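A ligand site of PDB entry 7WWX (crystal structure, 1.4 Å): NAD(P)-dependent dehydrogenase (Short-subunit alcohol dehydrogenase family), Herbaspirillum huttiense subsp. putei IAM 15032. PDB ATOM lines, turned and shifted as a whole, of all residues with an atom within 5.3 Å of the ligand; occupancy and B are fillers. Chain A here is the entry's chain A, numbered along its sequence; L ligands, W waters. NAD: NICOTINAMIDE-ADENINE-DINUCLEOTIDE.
An oxygen (O7N) of the ligand lies close to the backbone carbonyl oxygen (O) of Gly 210, 3.4 Å away.
Residues that only touch the ligand: Gly 36 (3.3 Å), Gly 40 (3.7 Å), Ile 61 (3.6 Å), Cys 86 (3.3 Å), Ala 115 (3.8 Å), Ala 116 (3.3 Å), Ile 137 (3.95 Å), Phe 164 (3.3 Å), Ser 165 (3.3 Å), Ser 166 (3.3 Å), Pro 209 (3.2 Å), Trp 211 (3.4 Å), Thr 214 (3.96 Å) and Gln 217 (3.7 Å).
Hydrophobic or aromatic side chains that line the ligand: Ile 41, Ile 61, Leu 88, Ala 115, Ala 116, Ile 137, Phe 164, Tyr 179, Pro 209, Trp 211 and Val 212.
25 residues have an atom within 4 Å of the ligand: Gly 36, Thr 39, Gly 40, Ile 41, Asp 60, Ile 61, Cys 86, Asp 87, Leu 88, Asn 114, Ala 115, Ala 116, Ile 137, Phe 164, Ser 165, Ser 166, Tyr 179, Lys 183, Pro 209, Gly 210, Trp 211, Val 212, Thr 214, Arg 216 and Gln 217.
The nearest printed residue that does not touch the ligand is Ala 62 (4.1 Å).
Water W2 lies within hydrogen-bond range of O1N of the ligand (2.5 Å), OG1 of Thr 214 (2.7 Å) and NE2 of Gln 217 (3.1 Å).
Water W6 lies within hydrogen-bond range of an oxygen (O2A) of the ligand (2.6 Å) and the side-chain hydroxyl (OG1) of Thr 39 (2.8 Å).
Water W7 lies within hydrogen-bond range of O1A of the ligand (2.6 Å), N of Asp 118 (3.0 Å) and NE of Arg 216 (3.2 Å).
Water W1 lies within hydrogen-bond range of an oxygen (O1A) of the ligand (2.8 Å), the side-chain amide nitrogen of Asn 117 (2.9 Å) and the backbone carbonyl oxygen of Ala 116 (3.1 Å).
Water W4 bridges OG of Ser 166 (2.5 Å) and OH of Tyr 179 (2.7 Å).
O3B of the ligand lies within hydrogen-bond range of OG1 of Thr 39, 2.6 Å away.
The side-chain carboxylate (OD1) of Asp 60 lies within hydrogen-bond range of an oxygen (O2B) of the ligand (2.6 Å).
The side-chain hydroxyl (OH) of Tyr 179 lies within hydrogen-bond range of an oxygen (O2D) of the ligand.
An oxygen (O3D) of the ligand lies within hydrogen-bond range of the backbone carbonyl oxygen of Asn 114 (2.8 Å).
An oxygen (O7N) of the ligand is in hydrogen-bond range of the backbone NH (N) of Val 212 (2.8 Å).
The backbone NH (N) of Ile 41 sits at hydrogen-bond distance from an oxygen (O2N) of the ligand.
An oxygen (O3D) of the ligand sits at hydrogen-bond distance from the side-chain amino group of Lys 183 (2.9 Å).
A nitrogen (N1A) of the ligand sits at hydrogen-bond distance from the backbone NH of Leu 88 (3.0 Å).
The side-chain carboxylate (OD1) of Asp 87 is in hydrogen-bond range of a nitrogen (N6A) of the ligand.
The guanidinium group (NE) of Arg 216 lies within salt-bridge range of an oxygen (O1A) of the ligand, at 3.7 Å.
The backbone carbonyl oxygen (O) of Asp 60 lies within hydrogen-bond range of the backbone NH (N) of Cys 86.
OD2 of Asp 60 is in hydrogen-bond range of N of Gly 38, 2.9 Å away.
N of Gly 37 sits at hydrogen-bond distance from OD2 of Asp 60, 3.4 Å away.
OG of Ser 165 is in hydrogen-bond range of O of Lys 183 (2.7 Å).
The backbone carbonyl oxygen of Phe 164 sits at hydrogen-bond distance from the side-chain amino group of Lys 183 (3.1 Å).
The backbone NH (N) of Ile 167 is in hydrogen-bond range of the backbone carbonyl oxygen (O) of Pro 209.
The backbone NH of Gly 36 lies within hydrogen-bond range of the backbone carbonyl oxygen of Val 59 (2.9 Å).
The backbone NH (N) of Gln 217 is in hydrogen-bond range of the side-chain hydroxyl (OG1) of Thr 214, at 3.0 Å.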
ATOM      1  N   GLY A  36       6.288   4.897 -16.245  1.00  0.00           N
ATOM      2  CA  GLY A  36       5.727   4.711 -14.910  1.00  0.00           C
ATOM      3  C   GLY A  36       4.652   3.629 -14.862  1.00  0.00           C
ATOM      4  O   GLY A  36       3.681   3.738 -14.109  1.00  0.00           O
ATOM      5  N   GLY A  37       4.909   2.483 -15.480  1.00  0.00           N
ATOM      6  CA  GLY A  37       3.893   1.432 -15.612  1.00  0.00           C
ATOM      7  C   GLY A  37       3.859   0.421 -14.499  1.00  0.00           C
ATOM      8  O   GLY A  37       2.997  -0.476 -14.558  1.00  0.00           O
ATOM      9  N   GLY A  38       4.711   0.541 -13.479  1.00  0.00           N
ATOM     10  CA  GLY A  38       4.850  -0.506 -12.435  1.00  0.00           C
ATOM     11  C   GLY A  38       3.805  -0.472 -11.355  1.00  0.00           C
ATOM     12  O   GLY A  38       3.595  -1.516 -10.690  1.00  0.00           O
ATOM     13  N   THR A  39       3.186   0.695 -11.085  1.00  0.00           N
ATOM     14  CA  THR A  39       2.282   0.867  -9.935  1.00  0.00           C
ATOM     15  C   THR A  39       1.209   1.904 -10.298  1.00  0.00           C
ATOM     16  O   THR A  39       1.289   2.492 -11.393  1.00  0.00           O
ATOM     17  CB  THR A  39       2.999   1.355  -8.678  1.00  0.00           C
ATOM     18  OG1 THR A  39       3.363   2.726  -8.869  1.00  0.00           O
ATOM     19  CG2 THR A  39       4.184   0.493  -8.279  1.00  0.00           C
ATOM     20  N   GLY A  40       0.157   2.000  -9.511  1.00  0.00           N
ATOM     21  CA  GLY A  40      -0.779   3.119  -9.667  1.00  0.00           C
ATOM     22  C   GLY A  40      -1.554   3.018 -10.967  1.00  0.00           C
ATOM     23  O   GLY A  40      -1.918   1.920 -11.472  1.00  0.00           O
ATOM     24  N   ILE A  41      -1.815   4.185 -11.545  1.00  0.00           N
ATOM     25  CA  ILE A  41      -2.589   4.211 -12.805  1.00  0.00           C
ATOM     26  C   ILE A  41      -1.783   3.500 -13.913  1.00  0.00           C
ATOM     27  O   ILE A  41      -2.372   2.778 -14.732  1.00  0.00           O
ATOM     28  CB  ILE A  41      -2.952   5.654 -13.177  1.00  0.00           C
ATOM     29  CG1 ILE A  41      -3.812   6.312 -12.094  1.00  0.00           C
ATOM     30  CG2 ILE A  41      -3.695   5.681 -14.492  1.00  0.00           C
ATOM     31  CD1 ILE A  41      -4.121   7.735 -12.335  1.00  0.00           C
ATOM     32  N   GLY A  42      -0.484   3.724 -13.971  1.00  0.00           N
ATOM     33  CA  GLY A  42       0.390   3.083 -14.948  1.00  0.00           C
ATOM     34  C   GLY A  42       0.200   1.574 -15.019  1.00  0.00           C
ATOM     35  O   GLY A  42       0.098   0.995 -16.066  1.00  0.00           O
ATOM     36  N   VAL A  59       8.763   1.432 -18.484  1.00  0.00           N
ATOM     37  CA  VAL A  59       9.874   1.764 -17.579  1.00  0.00           C
ATOM     38  C   VAL A  59       9.286   2.168 -16.235  1.00  0.00           C
ATOM     39  O   VAL A  59       8.149   2.731 -16.146  1.00  0.00           O
ATOM     40  CB  VAL A  59      10.811   2.836 -18.147  1.00  0.00           C
ATOM     41  CG1 VAL A  59      11.561   2.334 -19.342  1.00  0.00           C
ATOM     42  CG2 VAL A  59      10.070   4.117 -18.445  1.00  0.00           C
ATOM     43  N   ASP A  60      10.051   1.933 -15.197  1.00  0.00           N
ATOM     44  CA  ASP A  60       9.725   2.341 -13.820  1.00  0.00           C
ATOM     45  C   ASP A  60      11.022   2.212 -13.005  1.00  0.00           C
ATOM     46  O   ASP A  60      11.959   1.584 -13.498  1.00  0.00           O
ATOM     47  CB  ASP A  60       8.603   1.503 -13.231  1.00  0.00           C
ATOM     48  CG  ASP A  60       7.757   2.281 -12.238  1.00  0.00           C
ATOM     49  OD1 ASP A  60       8.270   2.655 -11.185  1.00  0.00           O
ATOM     50  OD2 ASP A  60       6.558   2.529 -12.554  1.00  0.00           O
ATOM     51  N   ILE A  61      11.029   2.801 -11.833  1.00  0.00           N
ATOM     52  CA  ILE A  61      12.114   2.580 -10.843  1.00  0.00           C
ATOM     53  C   ILE A  61      11.672   1.596  -9.780  1.00  0.00           C
ATOM     54  O   ILE A  61      12.559   1.149  -9.010  1.00  0.00           O
ATOM     55  CB  ILE A  61      12.582   3.905 -10.218  1.00  0.00           C
ATOM     56  CG1 ILE A  61      11.415   4.743  -9.704  1.00  0.00           C
ATOM     57  CG2 ILE A  61      13.476   4.631 -11.209  1.00  0.00           C
ATOM     58  CD1 ILE A  61      11.870   5.987  -8.965  1.00  0.00           C
ATOM     59  N   ALA A  62      10.399   1.169  -9.752  1.00  0.00           N
ATOM     60  CA  ALA A  62       9.879   0.267  -8.699  1.00  0.00           C
ATOM     61  C   ALA A  62      10.046  -1.183  -9.195  1.00  0.00           C
ATOM     62  O   ALA A  62       9.101  -1.778  -9.718  1.00  0.00           O
ATOM     63  CB  ALA A  62       8.449   0.640  -8.356  1.00  0.00           C
ATOM     64  N   CYS A  86      14.399   2.080 -15.278  1.00  0.00           N
ATOM     65  CA  CYS A  86      15.023   3.301 -15.816  1.00  0.00           C
ATOM     66  C   CYS A  86      14.532   4.498 -15.006  1.00  0.00           C
ATOM     67  O   CYS A  86      13.316   4.594 -14.815  1.00  0.00           O
ATOM     68  CB  CYS A  86      14.769   3.486 -17.306  1.00  0.00           C
ATOM     69  SG  CYS A  86      15.945   4.673 -18.011  1.00  0.00           S
ATOM     70  N   ASP A  87      15.458   5.323 -14.530  1.00  0.00           N
ATOM     71  CA  ASP A  87      15.130   6.619 -13.905  1.00  0.00           C
ATOM     72  C   ASP A  87      14.885   7.616 -15.024  1.00  0.00           C
ATOM     73  O   ASP A  87      15.837   7.958 -15.808  1.00  0.00           O
ATOM     74  CB  ASP A  87      16.259   7.046 -12.968  1.00  0.00           C
ATOM     75  CG  ASP A  87      15.882   8.200 -12.087  1.00  0.00           C
ATOM     76  OD1 ASP A  87      15.018   9.035 -12.516  1.00  0.00           O
ATOM     77  OD2 ASP A  87      16.421   8.280 -10.969  1.00  0.00           O
ATOM     78  N   LEU A  88      13.648   8.109 -15.114  1.00  0.00           N
ATOM     79  CA  LEU A  88      13.243   9.023 -16.211  1.00  0.00           C
ATOM     80  C   LEU A  88      13.993  10.368 -16.131  1.00  0.00           C
ATOM     81  O   LEU A  88      14.002  11.059 -17.151  1.00  0.00           O
ATOM     82  CB  LEU A  88      11.739   9.283 -16.056  1.00  0.00           C
ATOM     83  CG  LEU A  88      10.853   8.102 -16.376  1.00  0.00           C
ATOM     84  CD1 LEU A  88       9.463   8.321 -15.771  1.00  0.00           C
ATOM     85  CD2 LEU A  88      10.808   7.834 -17.859  1.00  0.00           C
ATOM     86  N   ARG A  89      14.586  10.683 -15.005  1.00  0.00           N
ATOM     87  CA  ARG A  89      15.426  11.892 -14.907  1.00  0.00           C
ATOM     88  C   ARG A  89      16.660  11.793 -15.790  1.00  0.00           C
ATOM     89  O   ARG A  89      17.228  12.851 -16.055  1.00  0.00           O
ATOM     90  CB  ARG A  89      15.787  12.164 -13.462  1.00  0.00           C
ATOM     91  CG  ARG A  89      14.586  12.369 -12.564  1.00  0.00           C
ATOM     92  CD  ARG A  89      14.940  12.662 -11.120  1.00  0.00           C
ATOM     93  NE  ARG A  89      15.649  11.500 -10.563  1.00  0.00           N
ATOM     94  CZ  ARG A  89      16.644  11.576  -9.681  1.00  0.00           C
ATOM     95  NH1 ARG A  89      17.043  12.741  -9.194  1.00  0.00           N
ATOM     96  NH2 ARG A  89      17.260  10.464  -9.303  1.00  0.00           N
ATOM     97  N   ASN A 113       2.416   8.624 -21.840  1.00  0.00           N
ATOM     98  CA  ASN A 113       3.222   9.437 -20.899  1.00  0.00           C
ATOM     99  C   ASN A 113       2.425   9.540 -19.610  1.00  0.00           C
ATOM    100  O   ASN A 113       1.614  10.468 -19.437  1.00  0.00           O
ATOM    101  CB  ASN A 113       3.543  10.779 -21.540  1.00  0.00           C
ATOM    102  CG  ASN A 113       4.695  10.690 -22.521  1.00  0.00           C
ATOM    103  OD1 ASN A 113       5.745  10.075 -22.191  1.00  0.00           O
ATOM    104  ND2 ASN A 113       4.582  11.415 -23.624  1.00  0.00           N
ATOM    105  N   ASN A 114       2.637   8.599 -18.707  1.00  0.00           N
ATOM    106  CA  ASN A 114       1.882   8.485 -17.426  1.00  0.00           C
ATOM    107  C   ASN A 114       2.706   8.934 -16.223  1.00  0.00           C
ATOM    108  O   ASN A 114       2.155   9.468 -15.291  1.00  0.00           O
ATOM    109  CB  ASN A 114       1.302   7.069 -17.324  1.00  0.00           C
ATOM    110  CG  ASN A 114       0.953   6.676 -15.910  1.00  0.00           C
ATOM    111  OD1 ASN A 114      -0.164   6.955 -15.450  1.00  0.00           O
ATOM    112  ND2 ASN A 114       1.899   6.084 -15.181  1.00  0.00           N
ATOM    113  N   ALA A 115       3.999   8.683 -16.185  1.00  0.00           N
ATOM    114  CA  ALA A 115       4.751   8.815 -14.958  1.00  0.00           C
ATOM    115  C   ALA A 115       4.662  10.254 -14.447  1.00  0.00           C
ATOM    116  O   ALA A 115       4.728  11.198 -15.242  1.00  0.00           O
ATOM    117  CB  ALA A 115       6.189   8.449 -15.176  1.00  0.00           C
ATOM    118  N   ALA A 116       4.620  10.400 -13.145  1.00  0.00           N
ATOM    119  CA  ALA A 116       4.641  11.714 -12.448  1.00  0.00           C
ATOM    120  C   ALA A 116       5.068  11.451 -11.010  1.00  0.00           C
ATOM    121  O   ALA A 116       5.142  10.274 -10.594  1.00  0.00           O
ATOM    122  CB  ALA A 116       3.274  12.361 -12.491  1.00  0.00           C
ATOM    123  N   ASN A 117       5.208  12.523 -10.266  1.00  0.00           N
ATOM    124  CA  ASN A 117       5.343  12.415  -8.794  1.00  0.00           C
ATOM    125  C   ASN A 117       4.751  13.674  -8.163  1.00  0.00           C
ATOM    126  O   ASN A 117       5.246  14.798  -8.479  1.00  0.00           O
ATOM    127  CB  ASN A 117       6.792  12.214  -8.352  1.00  0.00           C
ATOM    128  CG  ASN A 117       6.882  12.119  -6.848  1.00  0.00           C
ATOM    129  OD1 ASN A 117       6.892  13.133  -6.165  1.00  0.00           O
ATOM    130  ND2 ASN A 117       6.832  10.890  -6.358  1.00  0.00           N
ATOM    131  N   ASP A 118       3.734  13.526  -7.316  1.00  0.00           N
ATOM    132  CA  ASP A 118       2.928  14.637  -6.761  1.00  0.00           C
ATOM    133  C   ASP A 118       3.373  15.022  -5.342  1.00  0.00           C
ATOM    134  O   ASP A 118       2.598  15.647  -4.622  1.00  0.00           O
ATOM    135  CB  ASP A 118       1.440  14.247  -6.815  1.00  0.00           C
ATOM    136  CG  ASP A 118       1.021  13.195  -5.814  1.00  0.00           C
ATOM    137  OD1 ASP A 118       1.916  12.671  -5.089  1.00  0.00           O
ATOM    138  OD2 ASP A 118      -0.203  12.931  -5.754  1.00  0.00           O
ATOM    139  N   ILE A 137      11.294  15.080 -13.423  1.00  0.00           N
ATOM    140  CA  ILE A 137      10.415  13.893 -13.190  1.00  0.00           C
ATOM    141  C   ILE A 137       9.093  14.079 -13.935  1.00  0.00           C
ATOM    142  O   ILE A 137       8.604  13.168 -14.614  1.00  0.00           O
ATOM    143  CB  ILE A 137      10.139  13.666 -11.708  1.00  0.00           C
ATOM    144  CG1 ILE A 137      11.406  13.352 -10.933  1.00  0.00           C
ATOM    145  CG2 ILE A 137       9.090  12.577 -11.533  1.00  0.00           C
ATOM    146  CD1 ILE A 137      11.248  13.618  -9.472  1.00  0.00           C
ATOM    147  N   PHE A 164      -0.553  12.570 -19.818  1.00  0.00           N
ATOM    148  CA  PHE A 164      -1.362  12.749 -18.566  1.00  0.00           C
ATOM    149  C   PHE A 164      -1.190  14.125 -17.967  1.00  0.00           C
ATOM    150  O   PHE A 164      -0.071  14.501 -17.609  1.00  0.00           O
ATOM    151  CB  PHE A 164      -1.017  11.678 -17.545  1.00  0.00           C
ATOM    152  CG  PHE A 164      -1.850  10.443 -17.695  1.00  0.00           C
ATOM    153  CD1 PHE A 164      -1.757   9.600 -18.784  1.00  0.00           C
ATOM    154  CD2 PHE A 164      -2.795  10.144 -16.753  1.00  0.00           C
ATOM    155  CE1 PHE A 164      -2.604   8.506 -18.916  1.00  0.00           C
ATOM    156  CE2 PHE A 164      -3.659   9.073 -16.887  1.00  0.00           C
ATOM    157  CZ  PHE A 164      -3.528   8.233 -17.957  1.00  0.00           C
ATOM    158  N   SER A 165      -2.300  14.820 -17.811  1.00  0.00           N
ATOM    159  CA  SER A 165      -2.390  16.044 -16.979  1.00  0.00           C
ATOM    160  C   SER A 165      -3.013  15.653 -15.641  1.00  0.00           C
ATOM    161  O   SER A 165      -2.784  14.513 -15.190  1.00  0.00           O
ATOM    162  CB  SER A 165      -3.094  17.105 -17.746  1.00  0.00           C
ATOM    163  OG  SER A 165      -3.065  18.346 -17.042  1.00  0.00           O
ATOM    164  N   SER A 166      -3.708  16.578 -14.995  1.00  0.00           N
ATOM    165  CA  SER A 166      -4.281  16.374 -13.663  1.00  0.00           C
ATOM    166  C   SER A 166      -5.361  17.404 -13.456  1.00  0.00           C
ATOM    167  O   SER A 166      -5.176  18.556 -13.852  1.00  0.00           O
ATOM    168  CB  SER A 166      -3.196  16.554 -12.632  1.00  0.00           C
ATOM    169  OG  SER A 166      -3.695  16.687 -11.321  1.00  0.00           O
ATOM    170  N   ILE A 167      -6.382  17.081 -12.674  1.00  0.00           N
ATOM    171  CA  ILE A 167      -7.355  18.127 -12.259  1.00  0.00           C
ATOM    172  C   ILE A 167      -6.684  19.131 -11.331  1.00  0.00           C
ATOM    173  O   ILE A 167      -7.284  20.173 -11.148  1.00  0.00           O
ATOM    174  CB  ILE A 167      -8.672  17.587 -11.657  1.00  0.00           C
ATOM    175  CG1 ILE A 167      -8.460  16.799 -10.364  1.00  0.00           C
ATOM    176  CG2 ILE A 167      -9.477  16.845 -12.705  1.00  0.00           C
ATOM    177  CD1 ILE A 167      -9.732  16.565  -9.544  1.00  0.00           C
ATOM    178  N   TYR A 179       4.277  21.256  -9.268  1.00  0.00           N
ATOM    179  CA  TYR A 179       3.487  20.129  -9.831  1.00  0.00           C
ATOM    180  C   TYR A 179       2.360  20.707 -10.700  1.00  0.00           C
ATOM    181  O   TYR A 179       2.162  20.158 -11.815  1.00  0.00           O
ATOM    182  CB  TYR A 179       2.933  19.252  -8.690  1.00  0.00           C
ATOM    183  CG  TYR A 179       2.137  18.047  -9.178  1.00  0.00           C
ATOM    184  CD1 TYR A 179       2.753  16.952  -9.751  1.00  0.00           C
ATOM    185  CD2 TYR A 179       0.774  18.047  -9.044  1.00  0.00           C
ATOM    186  CE1 TYR A 179       2.019  15.852 -10.157  1.00  0.00           C
ATOM    187  CE2 TYR A 179       0.038  16.946  -9.441  1.00  0.00           C
ATOM    188  CZ  TYR A 179       0.665  15.859 -10.011  1.00  0.00           C
ATOM    189  OH  TYR A 179      -0.102  14.748 -10.363  1.00  0.00           O
ATOM    190  N   LYS A 183       1.887  19.935 -14.640  1.00  0.00           N
ATOM    191  CA  LYS A 183       0.653  19.270 -15.104  1.00  0.00           C
ATOM    192  C   LYS A 183      -0.086  20.128 -16.120  1.00  0.00           C
ATOM    193  O   LYS A 183      -0.618  19.568 -17.109  1.00  0.00           O
ATOM    194  CB  LYS A 183      -0.259  18.914 -13.945  1.00  0.00           C
ATOM    195  CG  LYS A 183       0.272  17.794 -13.074  1.00  0.00           C
ATOM    196  CD  LYS A 183       0.195  16.456 -13.764  1.00  0.00           C
ATOM    197  CE  LYS A 183       1.515  15.891 -14.164  1.00  0.00           C
ATOM    198  NZ  LYS A 183       1.294  14.594 -14.880  1.00  0.00           N
ATOM    199  N   PRO A 209      -6.940  12.878 -15.174  1.00  0.00           N
ATOM    200  CA  PRO A 209      -7.630  12.226 -14.064  1.00  0.00           C
ATOM    201  C   PRO A 209      -8.105  13.223 -13.010  1.00  0.00           C
ATOM    202  O   PRO A 209      -7.440  14.178 -12.680  1.00  0.00           O
ATOM    203  CB  PRO A 209      -6.605  11.303 -13.466  1.00  0.00           C
ATOM    204  CG  PRO A 209      -5.531  11.231 -14.513  1.00  0.00           C
ATOM    205  CD  PRO A 209      -5.512  12.574 -15.184  1.00  0.00           C
ATOM    206  N   GLY A 210      -9.194  12.821 -12.360  1.00  0.00           N
ATOM    207  CA  GLY A 210      -9.612  13.349 -11.054  1.00  0.00           C
ATOM    208  C   GLY A 210      -8.805  12.726  -9.946  1.00  0.00           C
ATOM    209  O   GLY A 210      -7.686  12.309 -10.150  1.00  0.00           O
ATOM    210  N   TRP A 211      -9.382  12.659  -8.758  1.00  0.00           N
ATOM    211  CA  TRP A 211      -8.644  12.112  -7.607  1.00  0.00           C
ATOM    212  C   TRP A 211      -8.793  10.607  -7.567  1.00  0.00           C
ATOM    213  O   TRP A 211      -9.824  10.098  -7.140  1.00  0.00           O
ATOM    214  CB  TRP A 211      -9.043  12.802  -6.326  1.00  0.00           C
ATOM    215  CG  TRP A 211      -7.999  12.619  -5.258  1.00  0.00           C
ATOM    216  CD1 TRP A 211      -6.773  12.006  -5.364  1.00  0.00           C
ATOM    217  CD2 TRP A 211      -8.054  13.138  -3.920  1.00  0.00           C
ATOM    218  NE1 TRP A 211      -6.102  12.059  -4.150  1.00  0.00           N
ATOM    219  CE2 TRP A 211      -6.856  12.765  -3.266  1.00  0.00           C
ATOM    220  CE3 TRP A 211      -9.016  13.879  -3.210  1.00  0.00           C
ATOM    221  CZ2 TRP A 211      -6.582  13.122  -1.946  1.00  0.00           C
ATOM    222  CZ3 TRP A 211      -8.748  14.238  -1.910  1.00  0.00           C
ATOM    223  CH2 TRP A 211      -7.556  13.849  -1.290  1.00  0.00           C
ATOM    224  N   VAL A 212      -7.813   9.927  -8.106  1.00  0.00           N
ATOM    225  CA  VAL A 212      -7.842   8.456  -8.347  1.00  0.00           C
ATOM    226  C   VAL A 212      -7.366   7.767  -7.065  1.00  0.00           C
ATOM    227  O   VAL A 212      -6.264   8.150  -6.557  1.00  0.00           O
ATOM    228  CB  VAL A 212      -7.006   8.078  -9.567  1.00  0.00           C
ATOM    229  CG1 VAL A 212      -7.056   6.560  -9.734  1.00  0.00           C
ATOM    230  CG2 VAL A 212      -7.440   8.771 -10.851  1.00  0.00           C
ATOM    231  N   THR A 214      -5.523   5.393  -5.901  1.00  0.00           N
ATOM    232  CA  THR A 214      -4.366   4.487  -5.930  1.00  0.00           C
ATOM    233  C   THR A 214      -3.942   4.232  -4.472  1.00  0.00           C
ATOM    234  O   THR A 214      -4.304   4.995  -3.546  1.00  0.00           O
ATOM    235  CB  THR A 214      -3.184   5.110  -6.677  1.00  0.00           C
ATOM    236  OG1 THR A 214      -2.776   6.234  -5.895  1.00  0.00           O
ATOM    237  CG2 THR A 214      -3.468   5.507  -8.116  1.00  0.00           C
ATOM    238  N   ARG A 216      -0.991   4.831  -3.349  1.00  0.00           N
ATOM    239  CA  ARG A 216      -0.196   6.028  -2.974  1.00  0.00           C
ATOM    240  C   ARG A 216      -1.146   7.091  -2.451  1.00  0.00           C
ATOM    241  O   ARG A 216      -0.836   7.769  -1.446  1.00  0.00           O
ATOM    242  CB  ARG A 216       0.614   6.571  -4.150  1.00  0.00           C
ATOM    243  CG  ARG A 216       1.340   7.877  -3.862  1.00  0.00           C
ATOM    244  CD  ARG A 216       2.173   8.357  -5.049  1.00  0.00           C
ATOM    245  NE  ARG A 216       2.647   9.716  -4.859  1.00  0.00           N
ATOM    246  CZ  ARG A 216       3.845  10.047  -4.356  1.00  0.00           C
ATOM    247  NH1 ARG A 216       4.675   9.074  -4.017  1.00  0.00           N
ATOM    248  NH2 ARG A 216       4.194  11.326  -4.219  1.00  0.00           N
ATOM    249  N   GLN A 217      -2.245   7.366  -3.164  1.00  0.00           N
ATOM    250  CA  GLN A 217      -3.115   8.475  -2.703  1.00  0.00           C
ATOM    251  C   GLN A 217      -3.695   8.145  -1.321  1.00  0.00           C
ATOM    252  O   GLN A 217      -3.782   9.044  -0.493  1.00  0.00           O
ATOM    253  CB  GLN A 217      -4.222   8.721  -3.716  1.00  0.00           C
ATOM    254  CG  GLN A 217      -3.683   9.244  -5.051  1.00  0.00           C
ATOM    255  CD  GLN A 217      -2.876  10.504  -4.904  1.00  0.00           C
ATOM    256  OE1 GLN A 217      -3.322  11.486  -4.337  1.00  0.00           O
ATOM    257  NE2 GLN A 217      -1.681  10.488  -5.462  1.00  0.00           N
HETATM  258  PA  NAD L   1       2.129   7.522  -8.917  1.00  0.00           P
HETATM  259  O1A NAD L   1       3.099   8.488  -8.289  1.00  0.00           O
HETATM  260  O2A NAD L   1       1.225   6.727  -8.035  1.00  0.00           O
HETATM  261  O5B NAD L   1       2.864   6.527  -9.928  1.00  0.00           O
HETATM  262  C5B NAD L   1       3.868   7.006 -10.824  1.00  0.00           C
HETATM  263  C4B NAD L   1       4.667   5.826 -11.295  1.00  0.00           C
HETATM  264  O4B NAD L   1       5.804   6.373 -12.026  1.00  0.00           O
HETATM  265  C3B NAD L   1       5.219   4.923 -10.198  1.00  0.00           C
HETATM  266  O3B NAD L   1       5.150   3.548 -10.531  1.00  0.00           O
HETATM  267  C2B NAD L   1       6.646   5.453 -10.043  1.00  0.00           C
HETATM  268  O2B NAD L   1       7.568   4.519  -9.508  1.00  0.00           O
HETATM  269  C1B NAD L   1       7.002   5.896 -11.451  1.00  0.00           C
HETATM  270  N9A NAD L   1       8.032   6.915 -11.421  1.00  0.00           N
HETATM  271  C8A NAD L   1       8.088   8.066 -10.657  1.00  0.00           C
HETATM  272  N7A NAD L   1       9.234   8.701 -10.776  1.00  0.00           N
HETATM  273  C5A NAD L   1       9.973   7.948 -11.676  1.00  0.00           C
HETATM  274  C6A NAD L   1      11.263   8.101 -12.222  1.00  0.00           C
HETATM  275  N6A NAD L   1      12.113   9.080 -11.873  1.00  0.00           N
HETATM  276  N1A NAD L   1      11.656   7.178 -13.113  1.00  0.00           N
HETATM  277  C2A NAD L   1      10.837   6.147 -13.398  1.00  0.00           C
HETATM  278  N3A NAD L   1       9.613   5.895 -12.949  1.00  0.00           N
HETATM  279  C4A NAD L   1       9.237   6.847 -12.072  1.00  0.00           C
HETATM  280  O3  NAD L   1       1.163   8.317  -9.921  1.00  0.00           O
HETATM  281  PN  NAD L   1      -0.342   8.056 -10.430  1.00  0.00           P
HETATM  282  O1N NAD L   1      -1.274   8.554  -9.363  1.00  0.00           O
HETATM  283  O2N NAD L   1      -0.450   6.578 -10.800  1.00  0.00           O
HETATM  284  O5D NAD L   1      -0.434   9.035 -11.663  1.00  0.00           O
HETATM  285  C5D NAD L   1      -0.222   8.650 -13.021  1.00  0.00           C
HETATM  286  C4D NAD L   1      -0.531   9.906 -13.816  1.00  0.00           C
HETATM  287  O4D NAD L   1      -1.865  10.396 -13.456  1.00  0.00           O
HETATM  288  C3D NAD L   1       0.429  11.070 -13.523  1.00  0.00           C
HETATM  289  O3D NAD L   1       0.750  11.778 -14.704  1.00  0.00           O
HETATM  290  C2D NAD L   1      -0.357  11.910 -12.524  1.00  0.00           C
HETATM  291  O2D NAD L   1       0.125  13.254 -12.498  1.00  0.00           O
HETATM  292  C1D NAD L   1      -1.756  11.734 -13.096  1.00  0.00           C
HETATM  293  N1N NAD L   1      -2.802  12.071 -12.096  1.00  0.00           N
HETATM  294  C2N NAD L   1      -3.035  11.224 -11.051  1.00  0.00           C
HETATM  295  C3N NAD L   1      -4.018  11.521 -10.143  1.00  0.00           C
HETATM  296  C7N NAD L   1      -4.353  10.672  -8.945  1.00  0.00           C
HETATM  297  O7N NAD L   1      -5.217  11.091  -8.188  1.00  0.00           O
HETATM  298  N7N NAD L   1      -3.696   9.533  -8.746  1.00  0.00           N
HETATM  299  C4N NAD L   1      -4.769  12.741 -10.325  1.00  0.00           C
HETATM  300  C5N NAD L   1      -4.568  13.517 -11.422  1.00  0.00           C
HETATM  301  C6N NAD L   1      -3.506  13.240 -12.241  1.00  0.00           C
HETATM  302  O   HOH W   1       5.838   8.672  -7.997  1.00  0.00           O
HETATM  303  O   HOH W   2      -0.950   7.886  -7.006  1.00  0.00           O
HETATM  304  O   HOH W   3      12.657  10.334  -9.058  1.00  0.00           O
HETATM  305  O   HOH W   4      -2.712  15.109  -9.616  1.00  0.00           O
HETATM  306  O   HOH W   5      -0.358  11.345  -8.976  1.00  0.00           O
HETATM  307  O   HOH W   6       2.011   4.442  -7.191  1.00  0.00           O
HETATM  308  O   HOH W   7       2.346  10.968  -7.802  1.00  0.00           O
HETATM  309  O   HOH W   8       1.349   5.239 -12.369  1.00  0.00           O
HETATM  310  O   HOH W   9      10.044   9.982  -8.366  1.00  0.00           O
